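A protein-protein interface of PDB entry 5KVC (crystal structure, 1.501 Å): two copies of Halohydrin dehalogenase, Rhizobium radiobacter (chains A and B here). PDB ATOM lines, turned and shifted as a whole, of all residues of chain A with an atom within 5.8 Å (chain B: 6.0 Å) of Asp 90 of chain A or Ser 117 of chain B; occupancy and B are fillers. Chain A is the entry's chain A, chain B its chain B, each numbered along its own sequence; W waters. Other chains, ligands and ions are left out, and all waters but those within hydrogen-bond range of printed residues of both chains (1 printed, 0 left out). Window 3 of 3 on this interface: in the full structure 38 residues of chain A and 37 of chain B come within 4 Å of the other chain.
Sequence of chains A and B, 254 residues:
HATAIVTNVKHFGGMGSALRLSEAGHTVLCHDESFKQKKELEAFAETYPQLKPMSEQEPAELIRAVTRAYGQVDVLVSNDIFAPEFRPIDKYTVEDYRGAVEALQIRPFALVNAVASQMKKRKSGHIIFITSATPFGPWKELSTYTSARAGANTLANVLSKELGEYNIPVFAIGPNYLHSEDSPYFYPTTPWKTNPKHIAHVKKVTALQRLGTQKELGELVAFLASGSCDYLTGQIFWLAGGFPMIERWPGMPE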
ATOM      1  N   PRO A  88     -24.790   2.683  -5.532  1.00  0.00           N
ATOM      2  CA  PRO A  88     -24.638   1.649  -6.548  1.00  0.00           C
ATOM      3  C   PRO A  88     -25.496   2.011  -7.750  1.00  0.00           C
ATOM      4  O   PRO A  88     -26.582   2.578  -7.609  1.00  0.00           O
ATOM      5  CB  PRO A  88     -25.145   0.377  -5.851  1.00  0.00           C
ATOM      6  CG  PRO A  88     -25.110   0.700  -4.394  1.00  0.00           C
ATOM      7  CD  PRO A  88     -25.332   2.149  -4.264  1.00  0.00           C
ATOM      8  N   ILE A  89     -24.990   1.693  -8.942  1.00  0.00           N
ATOM      9  CA  ILE A  89     -25.655   2.108 -10.178  1.00  0.00           C
ATOM     10  C   ILE A  89     -27.132   1.699 -10.203  1.00  0.00           C
ATOM     11  O   ILE A  89     -27.985   2.476 -10.654  1.00  0.00           O
ATOM     12  CB  ILE A  89     -24.874   1.547 -11.382  1.00  0.00           C
ATOM     13  CG1 ILE A  89     -25.536   1.922 -12.710  1.00  0.00           C
ATOM     14  CG2 ILE A  89     -24.723   0.016 -11.301  1.00  0.00           C
ATOM     15  CD1 ILE A  89     -25.730   3.393 -12.911  1.00  0.00           C
ATOM     16  N   ASP A  90     -27.472   0.489  -9.715  1.00  0.00           N
ATOM     17  CA  ASP A  90     -28.877   0.055  -9.802  1.00  0.00           C
ATOM     18  C   ASP A  90     -29.775   0.704  -8.745  1.00  0.00           C
ATOM     19  O   ASP A  90     -31.008   0.581  -8.844  1.00  0.00           O
ATOM     20  CB  ASP A  90     -28.981  -1.473  -9.682  1.00  0.00           C
ATOM     21  CG  ASP A  90     -28.272  -2.015  -8.454  1.00  0.00           C
ATOM     22  OD1 ASP A  90     -27.063  -1.738  -8.238  1.00  0.00           O
ATOM     23  OD2 ASP A  90     -28.932  -2.752  -7.661  1.00  0.00           O
ATOM     24  N   LYS A  91     -29.210   1.421  -7.782  1.00  0.00           N
ATOM     25  CA  LYS A  91     -30.010   2.069  -6.749  1.00  0.00           C
ATOM     26  C   LYS A  91     -30.361   3.516  -7.080  1.00  0.00           C
ATOM     27  O   LYS A  91     -31.254   4.090  -6.442  1.00  0.00           O
ATOM     28  CB  LYS A  91     -29.298   1.997  -5.388  1.00  0.00           C
ATOM     29  CG  LYS A  91     -29.073   0.568  -4.939  1.00  0.00           C
ATOM     30  CD  LYS A  91     -30.391  -0.166  -4.781  1.00  0.00           C
ATOM     31  CE  LYS A  91     -30.158  -1.597  -4.304  1.00  0.00           C
ATOM     32  NZ  LYS A  91     -31.435  -2.367  -4.240  1.00  0.00           N
ATOM     33  N   TYR A  92     -29.713   4.127  -8.071  1.00  0.00           N
ATOM     34  CA  TYR A  92     -30.219   5.389  -8.584  1.00  0.00           C
ATOM     35  C   TYR A  92     -31.538   5.179  -9.318  1.00  0.00           C
ATOM     36  O   TYR A  92     -31.882   4.064  -9.733  1.00  0.00           O
ATOM     37  CB  TYR A  92     -29.253   5.994  -9.620  1.00  0.00           C
ATOM     38  CG  TYR A  92     -27.908   6.480  -9.115  1.00  0.00           C
ATOM     39  CD1 TYR A  92     -27.802   7.593  -8.310  1.00  0.00           C
ATOM     40  CD2 TYR A  92     -26.719   5.846  -9.536  1.00  0.00           C
ATOM     41  CE1 TYR A  92     -26.552   8.061  -7.890  1.00  0.00           C
ATOM     42  CE2 TYR A  92     -25.513   6.292  -9.130  1.00  0.00           C
ATOM     43  CZ  TYR A  92     -25.409   7.385  -8.305  1.00  0.00           C
ATOM     44  OH  TYR A  92     -24.179   7.874  -7.898  1.00  0.00           O
ATOM     45  N   VAL B 112     -27.768   0.047 -17.909  1.00  0.00           N
ATOM     46  CA  VAL B 112     -26.990  -0.544 -16.819  1.00  0.00           C
ATOM     47  C   VAL B 112     -27.793  -0.515 -15.520  1.00  0.00           C
ATOM     48  O   VAL B 112     -27.744  -1.462 -14.724  1.00  0.00           O
ATOM     49  CB  VAL B 112     -25.631   0.173 -16.649  1.00  0.00           C
ATOM     50  CG1 VAL B 112     -24.830  -0.487 -15.527  1.00  0.00           C
ATOM     51  CG2 VAL B 112     -24.796   0.094 -17.931  1.00  0.00           C
ATOM     52  N   ASN B 113     -28.487   0.595 -15.270  1.00  0.00           N
ATOM     53  CA  ASN B 113     -29.355   0.736 -14.103  1.00  0.00           C
ATOM     54  C   ASN B 113     -30.390  -0.382 -14.052  1.00  0.00           C
ATOM     55  O   ASN B 113     -30.696  -0.880 -12.960  1.00  0.00           O
ATOM     56  CB  ASN B 113     -30.015   2.124 -14.141  1.00  0.00           C
ATOM     57  CG  ASN B 113     -31.041   2.326 -13.055  1.00  0.00           C
ATOM     58  OD1 ASN B 113     -32.250   2.276 -13.319  1.00  0.00           O
ATOM     59  ND2 ASN B 113     -30.582   2.598 -11.834  1.00  0.00           N
ATOM     60  N   ALA B 114     -30.840  -0.869 -15.208  1.00  0.00           N
ATOM     61  CA  ALA B 114     -31.852  -1.930 -15.219  1.00  0.00           C
ATOM     62  C   ALA B 114     -31.276  -3.341 -15.135  1.00  0.00           C
ATOM     63  O   ALA B 114     -31.982  -4.260 -14.676  1.00  0.00           O
ATOM     64  CB  ALA B 114     -32.696  -1.797 -16.486  1.00  0.00           C
ATOM     65  N   VAL B 115     -30.022  -3.557 -15.562  1.00  0.00           N
ATOM     66  CA  VAL B 115     -29.459  -4.898 -15.639  1.00  0.00           C
ATOM     67  C   VAL B 115     -28.459  -5.176 -14.510  1.00  0.00           C
ATOM     68  O   VAL B 115     -28.155  -6.353 -14.252  1.00  0.00           O
ATOM     69  CB  VAL B 115     -28.804  -5.172 -17.007  1.00  0.00           C
ATOM     70  CG1 VAL B 115     -27.419  -4.525 -17.090  1.00  0.00           C
ATOM     71  CG2 VAL B 115     -28.749  -6.679 -17.288  1.00  0.00           C
ATOM     72  N   ALA B 116     -27.969  -4.152 -13.815  1.00  0.00           N
ATOM     73  CA  ALA B 116     -26.836  -4.380 -12.916  1.00  0.00           C
ATOM     74  C   ALA B 116     -27.192  -5.304 -11.755  1.00  0.00           C
ATOM     75  O   ALA B 116     -26.359  -6.120 -11.337  1.00  0.00           O
ATOM     76  CB  ALA B 116     -26.303  -3.048 -12.373  1.00  0.00           C
ATOM     77  N   SER B 117     -28.405  -5.193 -11.212  1.00  0.00           N
ATOM     78  CA  SER B 117     -28.710  -5.974 -10.019  1.00  0.00           C
ATOM     79  C   SER B 117     -28.616  -7.472 -10.292  1.00  0.00           C
ATOM     80  O   SER B 117     -28.046  -8.213  -9.485  1.00  0.00           O
ATOM     81  CB  SER B 117     -30.084  -5.611  -9.467  1.00  0.00           C
ATOM     82  OG  SER B 117     -30.331  -6.411  -8.318  1.00  0.00           O
ATOM     83  N   GLN B 118     -29.151  -7.943 -11.425  1.00  0.00           N
ATOM     84  CA  GLN B 118     -29.055  -9.379 -11.709  1.00  0.00           C
ATOM     85  C   GLN B 118     -27.611  -9.823 -11.926  1.00  0.00           C
ATOM     86  O   GLN B 118     -27.225 -10.917 -11.501  1.00  0.00           O
ATOM     87  CB  GLN B 118     -29.930  -9.784 -12.893  1.00  0.00           C
ATOM     88  CG  GLN B 118     -29.542  -9.202 -14.254  1.00  0.00           C
ATOM     89  CD  GLN B 118     -30.222  -9.962 -15.360  1.00  0.00           C
ATOM     90  OE1 GLN B 118     -29.689 -10.932 -15.903  1.00  0.00           O
ATOM     91  NE2 GLN B 118     -31.409  -9.506 -15.719  1.00  0.00           N
ATOM     92  N   MET B 119     -26.791  -8.997 -12.585  1.00  0.00           N
ATOM     93  CA  MET B 119     -25.385  -9.354 -12.747  1.00  0.00           C
ATOM     94  C   MET B 119     -24.666  -9.386 -11.402  1.00  0.00           C
ATOM     95  O   MET B 119     -23.836 -10.272 -11.153  1.00  0.00           O
ATOM     96  CB  MET B 119     -24.700  -8.343 -13.688  1.00  0.00           C
ATOM     97  CG  MET B 119     -25.217  -8.351 -15.084  1.00  0.00           C
ATOM     98  SD  MET B 119     -24.241  -7.171 -16.096  1.00  0.00           S
ATOM     99  CE  MET B 119     -24.801  -7.578 -17.740  1.00  0.00           C
ATOM    100  N   LYS B 120     -24.953  -8.423 -10.531  1.00  0.00           N
ATOM    101  CA  LYS B 120     -24.299  -8.382  -9.235  1.00  0.00           C
ATOM    102  C   LYS B 120     -24.691  -9.583  -8.384  1.00  0.00           C
ATOM    103  O   LYS B 120     -23.842 -10.143  -7.683  1.00  0.00           O
ATOM    104  CB  LYS B 120     -24.646  -7.073  -8.535  1.00  0.00           C
ATOM    105  CG  LYS B 120     -23.911  -5.848  -9.171  1.00  0.00           C
ATOM    106  CD  LYS B 120     -24.541  -4.527  -8.784  1.00  0.00           C
ATOM    107  CE  LYS B 120     -24.582  -4.326  -7.304  1.00  0.00           C
ATOM    108  NZ  LYS B 120     -25.008  -2.957  -6.961  1.00  0.00           N
ATOM    109  N   LYS B 121     -25.964  -9.997  -8.445  1.00  0.00           N
ATOM    110  CA  LYS B 121     -26.417 -11.083  -7.573  1.00  0.00           C
ATOM    111  C   LYS B 121     -25.665 -12.367  -7.874  1.00  0.00           C
ATOM    112  O   LYS B 121     -25.292 -13.109  -6.954  1.00  0.00           O
ATOM    113  CB  LYS B 121     -27.922 -11.299  -7.722  1.00  0.00           C
ATOM    114  CG  LYS B 121     -28.482 -12.385  -6.792  1.00  0.00           C
ATOM    115  CD  LYS B 121     -30.005 -12.349  -6.761  1.00  0.00           C
ATOM    116  CE  LYS B 121     -30.576 -13.284  -5.700  1.00  0.00           C
ATOM    117  NZ  LYS B 121     -32.061 -13.126  -5.647  1.00  0.00           N
ATOM    118  N   ARG B 122     -25.412 -12.638  -9.147  1.00  0.00           N
ATOM    119  CA  ARG B 122     -24.678 -13.823  -9.538  1.00  0.00           C
ATOM    120  C   ARG B 122     -23.188 -13.572  -9.703  1.00  0.00           C
ATOM    121  O   ARG B 122     -22.453 -14.521  -9.978  1.00  0.00           O
ATOM    122  CB  ARG B 122     -25.253 -14.417 -10.819  1.00  0.00           C
ATOM    123  CG  ARG B 122     -25.114 -13.528 -11.973  1.00  0.00           C
ATOM    124  CD  ARG B 122     -25.727 -14.102 -13.243  1.00  0.00           C
ATOM    125  NE  ARG B 122     -25.266 -13.214 -14.311  1.00  0.00           N
ATOM    126  CZ  ARG B 122     -26.033 -12.414 -15.041  1.00  0.00           C
ATOM    127  NH1 ARG B 122     -27.357 -12.386 -14.897  1.00  0.00           N
ATOM    128  NH2 ARG B 122     -25.446 -11.638 -15.933  1.00  0.00           N
ATOM    129  N   GLU B 162     -16.982   0.291  -9.289  1.00  0.00           N
ATOM    130  CA  GLU B 162     -17.899  -0.380  -8.368  1.00  0.00           C
ATOM    131  C   GLU B 162     -18.221  -1.797  -8.800  1.00  0.00           C
ATOM    132  O   GLU B 162     -18.437  -2.674  -7.942  1.00  0.00           O
ATOM    133  CB  GLU B 162     -19.206   0.427  -8.209  1.00  0.00           C
ATOM    134  CG  GLU B 162     -20.081   0.410  -9.470  1.00  0.00           C
ATOM    135  CD  GLU B 162     -21.240   1.379  -9.350  1.00  0.00           C
ATOM    136  OE1 GLU B 162     -22.324   0.939  -8.873  1.00  0.00           O
ATOM    137  OE2 GLU B 162     -21.052   2.593  -9.636  1.00  0.00           O
HETATM  138  O   HOH W   1     -32.756  -0.240 -10.910  1.00  0.00           O
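Hydrophobic or aromatic side chains of chain A within 4 Å of the printed part of chain B: Pro 88 and Ile 89. Among the printed residues, 10 pairs touch across the chains. Among the printed residues, Asp or Glu carboxylates within 4 Å of a Lys or Arg side-chain nitrogen of the other chain: Asp 90 of chain A with Lys 120 of chain B (2.7 Å).
CB of Pro 88 of chain A touches NZ of Lys 120 of chain B (3.5 Å). Glu 162 of chain B touches Pro 88 of chain A. Val 112 of chain B touches Ile 89 of chain A. Ile 89 of chain A touches Ala 116 of chain B. Asp 90 of chain A touches Asn 113 of chain B (O to ND2, 3.6 Å). OD2 of Asp 90 of chain A touches CB of Ser 117 of chain B, 3.6 Å away.
The side-chain amino group of Lys 120 of chain B lies within salt-bridge range of the side-chain carboxylate of Asp 90 of chain A (2.7 Å). The backbone carbonyl oxygen of Tyr 92 of chain A lies within hydrogen-bond range of the side-chain amide nitrogen of Asn 113 of chain B (2.9 Å). The side-chain carboxylate of Glu 162 of chain B is in hydrogen-bond range of the backbone NH of Ile 89 of chain A, 2.8 Å away. The side-chain amide nitrogen of Asn 113 of chain B sits at hydrogen-bond distance from the backbone carbonyl oxygen of Ile 89 of chain A (2.9 Å).
No position is printed for both chains.
Water W1 lies within hydrogen-bond range of the backbone carbonyl oxygen (O) of Asp 90 of chain A (2.8 Å) and the backbone carbonyl oxygen (O) of Asn 113 of chain B (3.0 Å).
Printed residues of chain B within 4 Å of Ile 89 of chain A: Val 112 (3.8 Å), Asn 113 (2.9 Å), Ala 116 (3.6 Å) and Glu 162 (2.8 Å). Of the printed residues of chain B, Asp 90 of chain A touches Asn 113 (3.6 Å), Ser 117 (3.6 Å) and Lys 120 (2.7 Å). Of the printed residues of chain B, Tyr 92 of chain A touches Asn 113. Of the printed residues of chain A, Ser 117 of chain B touches Asp 90. Of the printed residues of chain A, Lys 120 of chain B touches Pro 88 (3.5 Å) and Asp 90 (2.7 Å). Printed residues of chain A within 4 Å of Glu 162 of chain B: Pro 88 and Ile 89. The nearest printed residue of chain B that does not touch Asp 90 of chain A is Ala 116 of chain B (4.1 Å). The nearest printed residue of chain A that does not touch Ser 117 of chain B is Lys 91 of chain A (5.8 Å).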
